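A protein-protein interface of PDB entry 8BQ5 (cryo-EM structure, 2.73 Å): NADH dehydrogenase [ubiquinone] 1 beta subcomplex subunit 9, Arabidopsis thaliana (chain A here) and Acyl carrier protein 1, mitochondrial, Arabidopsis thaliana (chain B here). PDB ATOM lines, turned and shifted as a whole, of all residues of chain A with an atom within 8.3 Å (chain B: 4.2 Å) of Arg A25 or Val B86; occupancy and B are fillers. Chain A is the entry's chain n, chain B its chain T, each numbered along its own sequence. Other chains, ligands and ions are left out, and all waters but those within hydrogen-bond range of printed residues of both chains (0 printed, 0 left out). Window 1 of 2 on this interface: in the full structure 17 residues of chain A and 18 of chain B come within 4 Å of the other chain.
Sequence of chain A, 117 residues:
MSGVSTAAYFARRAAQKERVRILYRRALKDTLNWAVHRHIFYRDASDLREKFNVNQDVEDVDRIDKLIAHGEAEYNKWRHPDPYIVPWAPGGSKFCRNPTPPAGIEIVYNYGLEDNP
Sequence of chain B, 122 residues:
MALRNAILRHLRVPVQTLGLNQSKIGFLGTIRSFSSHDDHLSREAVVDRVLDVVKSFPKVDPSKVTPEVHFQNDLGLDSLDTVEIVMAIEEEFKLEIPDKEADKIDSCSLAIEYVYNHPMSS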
ATOM      1  N   GLU A  18       6.357 -30.370  21.244  1.00  0.00           N
ATOM      2  CA  GLU A  18       5.731 -29.320  20.447  1.00  0.00           C
ATOM      3  C   GLU A  18       6.732 -28.227  20.089  1.00  0.00           C
ATOM      4  O   GLU A  18       6.730 -27.718  18.961  1.00  0.00           O
ATOM      5  CB  GLU A  18       4.533 -28.740  21.198  1.00  0.00           C
ATOM      6  CG  GLU A  18       4.223 -27.292  20.871  1.00  0.00           C
ATOM      7  CD  GLU A  18       2.807 -26.906  21.246  1.00  0.00           C
ATOM      8  OE1 GLU A  18       2.631 -25.862  21.908  1.00  0.00           O
ATOM      9  OE2 GLU A  18       1.872 -27.645  20.875  1.00  0.00           O
ATOM     10  N   ARG A  19       7.600 -27.859  21.035  1.00  0.00           N
ATOM     11  CA  ARG A  19       8.619 -26.851  20.759  1.00  0.00           C
ATOM     12  C   ARG A  19       9.564 -27.315  19.657  1.00  0.00           C
ATOM     13  O   ARG A  19       9.882 -26.557  18.732  1.00  0.00           O
ATOM     14  CB  ARG A  19       9.404 -26.541  22.035  1.00  0.00           C
ATOM     15  CG  ARG A  19       8.576 -25.970  23.177  1.00  0.00           C
ATOM     16  CD  ARG A  19       8.417 -24.464  23.054  1.00  0.00           C
ATOM     17  NE  ARG A  19       9.699 -23.774  23.117  1.00  0.00           N
ATOM     18  CZ  ARG A  19      10.373 -23.533  24.234  1.00  0.00           C
ATOM     19  NH1 ARG A  19       9.907 -23.901  25.416  1.00  0.00           N
ATOM     20  NH2 ARG A  19      11.543 -22.906  24.163  1.00  0.00           N
ATOM     21  N   VAL A  20      10.018 -28.567  19.737  1.00  0.00           N
ATOM     22  CA  VAL A  20      10.982 -29.088  18.770  1.00  0.00           C
ATOM     23  C   VAL A  20      10.357 -29.171  17.382  1.00  0.00           C
ATOM     24  O   VAL A  20      11.003 -28.873  16.370  1.00  0.00           O
ATOM     25  CB  VAL A  20      11.516 -30.455  19.236  1.00  0.00           C
ATOM     26  CG1 VAL A  20      12.366 -31.104  18.157  1.00  0.00           C
ATOM     27  CG2 VAL A  20      12.314 -30.293  20.519  1.00  0.00           C
ATOM     28  N   ARG A  21       9.090 -29.584  17.314  1.00  0.00           N
ATOM     29  CA  ARG A  21       8.419 -29.702  16.023  1.00  0.00           C
ATOM     30  C   ARG A  21       8.260 -28.341  15.358  1.00  0.00           C
ATOM     31  O   ARG A  21       8.426 -28.212  14.140  1.00  0.00           O
ATOM     32  CB  ARG A  21       7.059 -30.368  16.207  1.00  0.00           C
ATOM     33  CG  ARG A  21       7.130 -31.830  16.600  1.00  0.00           C
ATOM     34  CD  ARG A  21       5.959 -32.596  16.026  1.00  0.00           C
ATOM     35  NE  ARG A  21       4.681 -32.082  16.504  1.00  0.00           N
ATOM     36  CZ  ARG A  21       4.186 -32.291  17.716  1.00  0.00           C
ATOM     37  NH1 ARG A  21       4.848 -32.986  18.626  1.00  0.00           N
ATOM     38  NH2 ARG A  21       2.994 -31.788  18.024  1.00  0.00           N
ATOM     39  N   ILE A  22       7.925 -27.316  16.143  1.00  0.00           N
ATOM     40  CA  ILE A  22       7.804 -25.962  15.612  1.00  0.00           C
ATOM     41  C   ILE A  22       9.163 -25.418  15.203  1.00  0.00           C
ATOM     42  O   ILE A  22       9.291 -24.742  14.175  1.00  0.00           O
ATOM     43  CB  ILE A  22       7.113 -25.056  16.647  1.00  0.00           C
ATOM     44  CG1 ILE A  22       5.658 -25.485  16.842  1.00  0.00           C
ATOM     45  CG2 ILE A  22       7.212 -23.593  16.240  1.00  0.00           C
ATOM     46  CD1 ILE A  22       4.949 -25.838  15.554  1.00  0.00           C
ATOM     47  N   LEU A  23      10.199 -25.700  15.994  1.00  0.00           N
ATOM     48  CA  LEU A  23      11.538 -25.240  15.649  1.00  0.00           C
ATOM     49  C   LEU A  23      12.002 -25.861  14.338  1.00  0.00           C
ATOM     50  O   LEU A  23      12.652 -25.200  13.520  1.00  0.00           O
ATOM     51  CB  LEU A  23      12.511 -25.562  16.782  1.00  0.00           C
ATOM     52  CG  LEU A  23      13.957 -25.153  16.519  1.00  0.00           C
ATOM     53  CD1 LEU A  23      14.030 -23.660  16.251  1.00  0.00           C
ATOM     54  CD2 LEU A  23      14.832 -25.525  17.698  1.00  0.00           C
ATOM     55  N   TYR A  24      11.675 -27.137  14.121  1.00  0.00           N
ATOM     56  CA  TYR A  24      11.972 -27.768  12.841  1.00  0.00           C
ATOM     57  C   TYR A  24      11.183 -27.120  11.710  1.00  0.00           C
ATOM     58  O   TYR A  24      11.707 -26.932  10.606  1.00  0.00           O
ATOM     59  CB  TYR A  24      11.672 -29.265  12.905  1.00  0.00           C
ATOM     60  CG  TYR A  24      12.077 -30.012  11.654  1.00  0.00           C
ATOM     61  CD1 TYR A  24      13.395 -30.007  11.217  1.00  0.00           C
ATOM     62  CD2 TYR A  24      11.139 -30.705  10.902  1.00  0.00           C
ATOM     63  CE1 TYR A  24      13.769 -30.681  10.074  1.00  0.00           C
ATOM     64  CE2 TYR A  24      11.504 -31.382   9.756  1.00  0.00           C
ATOM     65  CZ  TYR A  24      12.820 -31.366   9.348  1.00  0.00           C
ATOM     66  OH  TYR A  24      13.191 -32.038   8.208  1.00  0.00           O
ATOM     67  N   ARG A  25       9.913 -26.789  11.960  1.00  0.00           N
ATOM     68  CA  ARG A  25       9.084 -26.199  10.915  1.00  0.00           C
ATOM     69  C   ARG A  25       9.617 -24.836  10.488  1.00  0.00           C
ATOM     70  O   ARG A  25       9.638 -24.514   9.295  1.00  0.00           O
ATOM     71  CB  ARG A  25       7.636 -26.088  11.394  1.00  0.00           C
ATOM     72  CG  ARG A  25       6.804 -25.035  10.674  1.00  0.00           C
ATOM     73  CD  ARG A  25       5.333 -25.429  10.632  1.00  0.00           C
ATOM     74  NE  ARG A  25       4.492 -24.401  10.029  1.00  0.00           N
ATOM     75  CZ  ARG A  25       3.956 -24.481   8.819  1.00  0.00           C
ATOM     76  NH1 ARG A  25       4.183 -25.516   8.028  1.00  0.00           N
ATOM     77  NH2 ARG A  25       3.175 -23.493   8.388  1.00  0.00           N
ATOM     78  N   ARG A  26      10.056 -24.024  11.451  1.00  0.00           N
ATOM     79  CA  ARG A  26      10.567 -22.699  11.117  1.00  0.00           C
ATOM     80  C   ARG A  26      11.952 -22.775  10.487  1.00  0.00           C
ATOM     81  O   ARG A  26      12.246 -22.044   9.533  1.00  0.00           O
ATOM     82  CB  ARG A  26      10.581 -21.814  12.363  1.00  0.00           C
ATOM     83  CG  ARG A  26       9.192 -21.504  12.900  1.00  0.00           C
ATOM     84  CD  ARG A  26       9.169 -20.196  13.668  1.00  0.00           C
ATOM     85  NE  ARG A  26       9.143 -20.401  15.112  1.00  0.00           N
ATOM     86  CZ  ARG A  26       8.066 -20.252  15.870  1.00  0.00           C
ATOM     87  NH1 ARG A  26       6.894 -19.923  15.351  1.00  0.00           N
ATOM     88  NH2 ARG A  26       8.166 -20.440  17.183  1.00  0.00           N
ATOM     89  N   ALA A  27      12.818 -23.652  11.002  1.00  0.00           N
ATOM     90  CA  ALA A  27      14.154 -23.780  10.430  1.00  0.00           C
ATOM     91  C   ALA A  27      14.089 -24.264   8.989  1.00  0.00           C
ATOM     92  O   ALA A  27      14.905 -23.862   8.151  1.00  0.00           O
ATOM     93  CB  ALA A  27      15.003 -24.728  11.277  1.00  0.00           C
ATOM     94  N   LEU A  28      13.120 -25.128   8.677  1.00  0.00           N
ATOM     95  CA  LEU A  28      13.033 -25.670   7.327  1.00  0.00           C
ATOM     96  C   LEU A  28      12.445 -24.651   6.357  1.00  0.00           C
ATOM     97  O   LEU A  28      12.677 -24.736   5.145  1.00  0.00           O
ATOM     98  CB  LEU A  28      12.209 -26.956   7.330  1.00  0.00           C
ATOM     99  CG  LEU A  28      12.639 -27.966   6.263  1.00  0.00           C
ATOM    100  CD1 LEU A  28      13.899 -28.642   6.650  1.00  0.00           C
ATOM    101  CD2 LEU A  28      11.590 -29.016   6.029  1.00  0.00           C
ATOM    102  N   LYS A  29      11.673 -23.685   6.862  1.00  0.00           N
ATOM    103  CA  LYS A  29      11.209 -22.604   5.998  1.00  0.00           C
ATOM    104  C   LYS A  29      12.275 -21.531   5.831  1.00  0.00           C
ATOM    105  O   LYS A  29      12.375 -20.921   4.761  1.00  0.00           O
ATOM    106  CB  LYS A  29       9.925 -21.987   6.546  1.00  0.00           C
ATOM    107  CG  LYS A  29       8.675 -22.804   6.275  1.00  0.00           C
ATOM    108  CD  LYS A  29       7.589 -22.475   7.282  1.00  0.00           C
ATOM    109  CE  LYS A  29       6.227 -22.923   6.786  1.00  0.00           C
ATOM    110  NZ  LYS A  29       5.306 -21.774   6.584  1.00  0.00           N
ATOM    111  N   ASP A  30      13.064 -21.318   6.887  1.00  0.00           N
ATOM    112  CA  ASP A  30      14.191 -20.362   6.792  1.00  0.00           C
ATOM    113  C   ASP A  30      15.219 -20.886   5.789  1.00  0.00           C
ATOM    114  O   ASP A  30      15.867 -20.054   5.138  1.00  0.00           O
ATOM    115  CB  ASP A  30      14.858 -20.152   8.145  1.00  0.00           C
ATOM    116  CG  ASP A  30      15.686 -18.886   8.184  1.00  0.00           C
ATOM    117  OD1 ASP A  30      16.900 -18.984   8.438  1.00  0.00           O
ATOM    118  OD2 ASP A  30      15.105 -17.818   7.934  1.00  0.00           O
ATOM    119  N   THR A  31      15.369 -22.208   5.684  1.00  0.00           N
ATOM    120  CA  THR A  31      16.356 -22.788   4.780  1.00  0.00           C
ATOM    121  C   THR A  31      16.050 -22.431   3.331  1.00  0.00           C
ATOM    122  O   THR A  31      16.958 -22.095   2.560  1.00  0.00           O
ATOM    123  CB  THR A  31      16.407 -24.305   4.962  1.00  0.00           C
ATOM    124  OG1 THR A  31      17.046 -24.615   6.205  1.00  0.00           O
ATOM    125  CG2 THR A  31      17.182 -24.960   3.826  1.00  0.00           C
ATOM    126  N   LEU A  48      19.949 -30.056   7.609  1.00  0.00           N
ATOM    127  CA  LEU A  48      19.220 -29.548   8.767  1.00  0.00           C
ATOM    128  C   LEU A  48      18.460 -30.670   9.471  1.00  0.00           C
ATOM    129  O   LEU A  48      18.473 -30.756  10.705  1.00  0.00           O
ATOM    130  CB  LEU A  48      18.276 -28.417   8.337  1.00  0.00           C
ATOM    131  CG  LEU A  48      16.986 -28.133   9.113  1.00  0.00           C
ATOM    132  CD1 LEU A  48      17.343 -27.493  10.414  1.00  0.00           C
ATOM    133  CD2 LEU A  48      16.112 -27.160   8.392  1.00  0.00           C
ATOM    134  N   PHE A  52      18.713 -32.460  13.586  1.00  0.00           N
ATOM    135  CA  PHE A  52      17.709 -32.886  14.556  1.00  0.00           C
ATOM    136  C   PHE A  52      17.800 -34.386  14.814  1.00  0.00           C
ATOM    137  O   PHE A  52      17.418 -34.864  15.887  1.00  0.00           O
ATOM    138  CB  PHE A  52      16.309 -32.514  14.069  1.00  0.00           C
ATOM    139  CG  PHE A  52      15.878 -31.127  14.451  1.00  0.00           C
ATOM    140  CD1 PHE A  52      16.297 -30.030  13.719  1.00  0.00           C
ATOM    141  CD2 PHE A  52      15.050 -30.920  15.544  1.00  0.00           C
ATOM    142  CE1 PHE A  52      15.901 -28.754  14.067  1.00  0.00           C
ATOM    143  CE2 PHE A  52      14.652 -29.646  15.897  1.00  0.00           C
ATOM    144  CZ  PHE A  52      15.078 -28.562  15.157  1.00  0.00           C
ATOM    145  N   TYR A  75      18.136 -20.412  15.509  1.00  0.00           N
ATOM    146  CA  TYR A  75      17.170 -19.954  14.481  1.00  0.00           C
ATOM    147  C   TYR A  75      17.057 -18.433  14.557  1.00  0.00           C
ATOM    148  O   TYR A  75      17.185 -17.791  13.507  1.00  0.00           O
ATOM    149  CB  TYR A  75      15.806 -20.618  14.666  1.00  0.00           C
ATOM    150  CG  TYR A  75      14.710 -20.027  13.817  1.00  0.00           C
ATOM    151  CD1 TYR A  75      13.647 -19.347  14.389  1.00  0.00           C
ATOM    152  CD2 TYR A  75      14.743 -20.135  12.436  1.00  0.00           C
ATOM    153  CE1 TYR A  75      12.645 -18.792  13.613  1.00  0.00           C
ATOM    154  CE2 TYR A  75      13.747 -19.587  11.647  1.00  0.00           C
ATOM    155  CZ  TYR A  75      12.695 -18.914  12.236  1.00  0.00           C
ATOM    156  OH  TYR A  75      11.710 -18.378  11.458  1.00  0.00           O
ATOM    157  N   THR B  82       6.267 -35.865   9.543  1.00  0.00           N
ATOM    158  CA  THR B  82       4.952 -35.253   9.374  1.00  0.00           C
ATOM    159  C   THR B  82       5.069 -33.786   8.983  1.00  0.00           C
ATOM    160  O   THR B  82       4.312 -33.302   8.133  1.00  0.00           O
ATOM    161  CB  THR B  82       4.144 -35.398  10.664  1.00  0.00           C
ATOM    162  OG1 THR B  82       4.095 -36.780  11.042  1.00  0.00           O
ATOM    163  CG2 THR B  82       2.730 -34.870  10.477  1.00  0.00           C
ATOM    164  N   VAL B  83       6.013 -33.066   9.593  1.00  0.00           N
ATOM    165  CA  VAL B  83       6.201 -31.651   9.285  1.00  0.00           C
ATOM    166  C   VAL B  83       6.531 -31.467   7.811  1.00  0.00           C
ATOM    167  O   VAL B  83       6.013 -30.558   7.149  1.00  0.00           O
ATOM    168  CB  VAL B  83       7.297 -31.054  10.187  1.00  0.00           C
ATOM    169  CG1 VAL B  83       7.587 -29.619   9.793  1.00  0.00           C
ATOM    170  CG2 VAL B  83       6.889 -31.147  11.649  1.00  0.00           C
ATOM    171  N   GLU B  84       7.400 -32.324   7.274  1.00  0.00           N
ATOM    172  CA  GLU B  84       7.717 -32.264   5.852  1.00  0.00           C
ATOM    173  C   GLU B  84       6.477 -32.509   5.006  1.00  0.00           C
ATOM    174  O   GLU B  84       6.289 -31.867   3.966  1.00  0.00           O
ATOM    175  CB  GLU B  84       8.810 -33.278   5.521  1.00  0.00           C
ATOM    176  CG  GLU B  84      10.154 -32.951   6.141  1.00  0.00           C
ATOM    177  CD  GLU B  84      10.893 -34.189   6.608  1.00  0.00           C
ATOM    178  OE1 GLU B  84      10.314 -35.291   6.530  1.00  0.00           O
ATOM    179  OE2 GLU B  84      12.050 -34.059   7.057  1.00  0.00           O
ATOM    180  N   ILE B  85       5.617 -33.434   5.437  1.00  0.00           N
ATOM    181  CA  ILE B  85       4.368 -33.679   4.724  1.00  0.00           C
ATOM    182  C   ILE B  85       3.494 -32.433   4.745  1.00  0.00           C
ATOM    183  O   ILE B  85       2.884 -32.068   3.733  1.00  0.00           O
ATOM    184  CB  ILE B  85       3.634 -34.894   5.321  1.00  0.00           C
ATOM    185  CG1 ILE B  85       4.550 -36.121   5.343  1.00  0.00           C
ATOM    186  CG2 ILE B  85       2.369 -35.195   4.535  1.00  0.00           C
ATOM    187  CD1 ILE B  85       5.326 -36.340   4.062  1.00  0.00           C
ATOM    188  N   VAL B  86       3.418 -31.761   5.894  1.00  0.00           N
ATOM    189  CA  VAL B  86       2.615 -30.548   5.993  1.00  0.00           C
ATOM    190  C   VAL B  86       3.162 -29.468   5.069  1.00  0.00           C
ATOM    191  O   VAL B  86       2.407 -28.826   4.331  1.00  0.00           O
ATOM    192  CB  VAL B  86       2.550 -30.070   7.456  1.00  0.00           C
ATOM    193  CG1 VAL B  86       1.885 -28.707   7.543  1.00  0.00           C
ATOM    194  CG2 VAL B  86       1.813 -31.086   8.310  1.00  0.00           C
ATOM    195  N   MET B  87       4.485 -29.273   5.072  1.00  0.00           N
ATOM    196  CA  MET B  87       5.095 -28.246   4.230  1.00  0.00           C
ATOM    197  C   MET B  87       4.832 -28.510   2.755  1.00  0.00           C
ATOM    198  O   MET B  87       4.572 -27.578   1.985  1.00  0.00           O
ATOM    199  CB  MET B  87       6.599 -28.171   4.495  1.00  0.00           C
ATOM    200  CG  MET B  87       7.220 -26.833   4.131  1.00  0.00           C
ATOM    201  SD  MET B  87       8.934 -26.668   4.662  1.00  0.00           S
ATOM    202  CE  MET B  87       9.776 -26.769   3.086  1.00  0.00           C
ATOM    203  N   ALA B  88       4.911 -29.775   2.336  1.00  0.00           N
ATOM    204  CA  ALA B  88       4.612 -30.108   0.949  1.00  0.00           C
ATOM    205  C   ALA B  88       3.126 -29.943   0.648  1.00  0.00           C
ATOM    206  O   ALA B  88       2.743 -29.726  -0.506  1.00  0.00           O
ATOM    207  CB  ALA B  88       5.079 -31.529   0.639  1.00  0.00           C
ATOM    208  N   ILE B  89       2.275 -30.057   1.670  1.00  0.00           N
ATOM    209  CA  ILE B  89       0.862 -29.730   1.491  1.00  0.00           C
ATOM    210  C   ILE B  89       0.687 -28.226   1.323  1.00  0.00           C
ATOM    211  O   ILE B  89      -0.114 -27.766   0.499  1.00  0.00           O
ATOM    212  CB  ILE B  89       0.025 -30.277   2.665  1.00  0.00           C
ATOM    213  CG1 ILE B  89      -0.126 -31.795   2.551  1.00  0.00           C
ATOM    214  CG2 ILE B  89      -1.345 -29.622   2.706  1.00  0.00           C
ATOM    215  CD1 ILE B  89      -0.307 -32.488   3.880  1.00  0.00           C
ATOM    216  N   GLU B  90       1.436 -27.436   2.098  1.00  0.00           N
ATOM    217  CA  GLU B  90       1.420 -25.987   1.927  1.00  0.00           C
ATOM    218  C   GLU B  90       1.843 -25.598   0.520  1.00  0.00           C
ATOM    219  O   GLU B  90       1.202 -24.762  -0.126  1.00  0.00           O
ATOM    220  CB  GLU B  90       2.352 -25.323   2.941  1.00  0.00           C
ATOM    221  CG  GLU B  90       2.196 -25.810   4.361  1.00  0.00           C
ATOM    222  CD  GLU B  90       1.437 -24.838   5.222  1.00  0.00           C
ATOM    223  OE1 GLU B  90       0.548 -24.146   4.687  1.00  0.00           O
ATOM    224  OE2 GLU B  90       1.733 -24.760   6.432  1.00  0.00           O
ATOM    225  N   ILE B  97      -0.147 -21.792   6.651  1.00  0.00           N
ATOM    226  CA  ILE B  97      -0.752 -22.174   7.928  1.00  0.00           C
ATOM    227  C   ILE B  97       0.066 -21.555   9.058  1.00  0.00           C
ATOM    228  O   ILE B  97       1.304 -21.546   8.980  1.00  0.00           O
ATOM    229  CB  ILE B  97      -0.811 -23.691   8.062  1.00  0.00           C
ATOM    230  CG1 ILE B  97      -1.586 -24.297   6.895  1.00  0.00           C
ATOM    231  CG2 ILE B  97      -1.472 -24.086   9.368  1.00  0.00           C
ATOM    232  CD1 ILE B  97      -1.463 -25.796   6.798  1.00  0.00           C
ATOM    233  N   ASP B  99       1.910 -21.482  12.708  1.00  0.00           N
ATOM    234  CA  ASP B  99       2.690 -22.546  13.333  1.00  0.00           C
ATOM    235  C   ASP B  99       1.880 -23.318  14.368  1.00  0.00           C
ATOM    236  O   ASP B  99       2.080 -24.526  14.534  1.00  0.00           O
ATOM    237  CB  ASP B  99       3.950 -21.963  13.968  1.00  0.00           C
ATOM    238  CG  ASP B  99       4.854 -21.297  12.954  1.00  0.00           C
ATOM    239  OD1 ASP B  99       4.481 -21.258  11.763  1.00  0.00           O
ATOM    240  OD2 ASP B  99       5.936 -20.813  13.344  1.00  0.00           O
ATOM    241  N   ALA B 102      -0.481 -25.635  12.410  1.00  0.00           N
ATOM    242  CA  ALA B 102       0.232 -26.603  11.582  1.00  0.00           C
ATOM    243  C   ALA B 102       0.634 -27.832  12.385  1.00  0.00           C
ATOM    244  O   ALA B 102       0.579 -28.960  11.881  1.00  0.00           O
ATOM    245  CB  ALA B 102       1.462 -25.954  10.949  1.00  0.00           C
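O of Ile B97 is in hydrogen-bond range of NH2 of Arg A25 (2.8 Å).
The side-chain carboxylate (OD2) of Asp B99 lies within salt-bridge range of the guanidinium group (NE) of Arg A26, 3.7 Å away.
The side-chain hydroxyl (OH) of Tyr A24 lies within hydrogen-bond range of the side-chain carboxylate (OE2) of Glu B84, at 2.6 Å.
The side-chain carboxylate (OE2) of Glu B90 is in salt-bridge range of the guanidinium group (NH2) of Arg A25 (2.7 Å).
NE of Arg A25 is in salt-bridge range of OD1 of Asp B99 (3.6 Å).
The backbone NH of Ile B97 lies close to the side-chain carboxylate of Glu B90 (3.1 Å).
O of Asp B99 touches CD1 of Ile A22 (3.3 Å).
CG1 of Val B83 touches CD2 of Tyr A24 (3.9 Å).
Arg A25 touches Val B83 (CB to CG1, 3.9 Å).
Arg A25 touches Val B86 (NH1 to CG1, 3.96 Å).
Arg A25 touches Ala B102 (NE to CB, 3.5 Å).
Leu A28 touches Met B87 (CD2 to SD, 3.8 Å).
Arg A25 touches just these residues of chain B: Val B83 (3.9 Å), Val B86 (3.96 Å), Glu B90 (2.7 Å), Ile B97 (2.8 Å), Asp B99 (3.6 Å) and Ala B102 (3.5 Å).
Of chain A, only Arg A25 comes within 4 Å of Val B86.
Printed residues of chain B within 4 Å of Tyr A24: Val B83 (3.9 Å) and Glu B84 (2.6 Å).
Of the printed residues of chain B, Arg A26 touches Asp B99.
Of the printed residues of chain A, Ala B102 touches Arg A25.
Of the printed residues of chain A, Met B87 touches Leu A28.
Arg A19 touches none of the printed residues of chain B.
Ile B89 touches none of the printed residues of chain A.
The nearest residue of chain A that does not touch Val B86 is Lys A29 (7.3 Å).
Of the 17 printed residues of chain A, 5 touch a printed residue of chain B.
Hydrophobic or aromatic side chains of chain A that line the printed part of chain B: Ile A22, Tyr A24 and Leu A28.
Hydrophobic or aromatic side chains of chain B that line the printed part of chain A: Val B83, Val B86, Met B87 and Ala B102.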
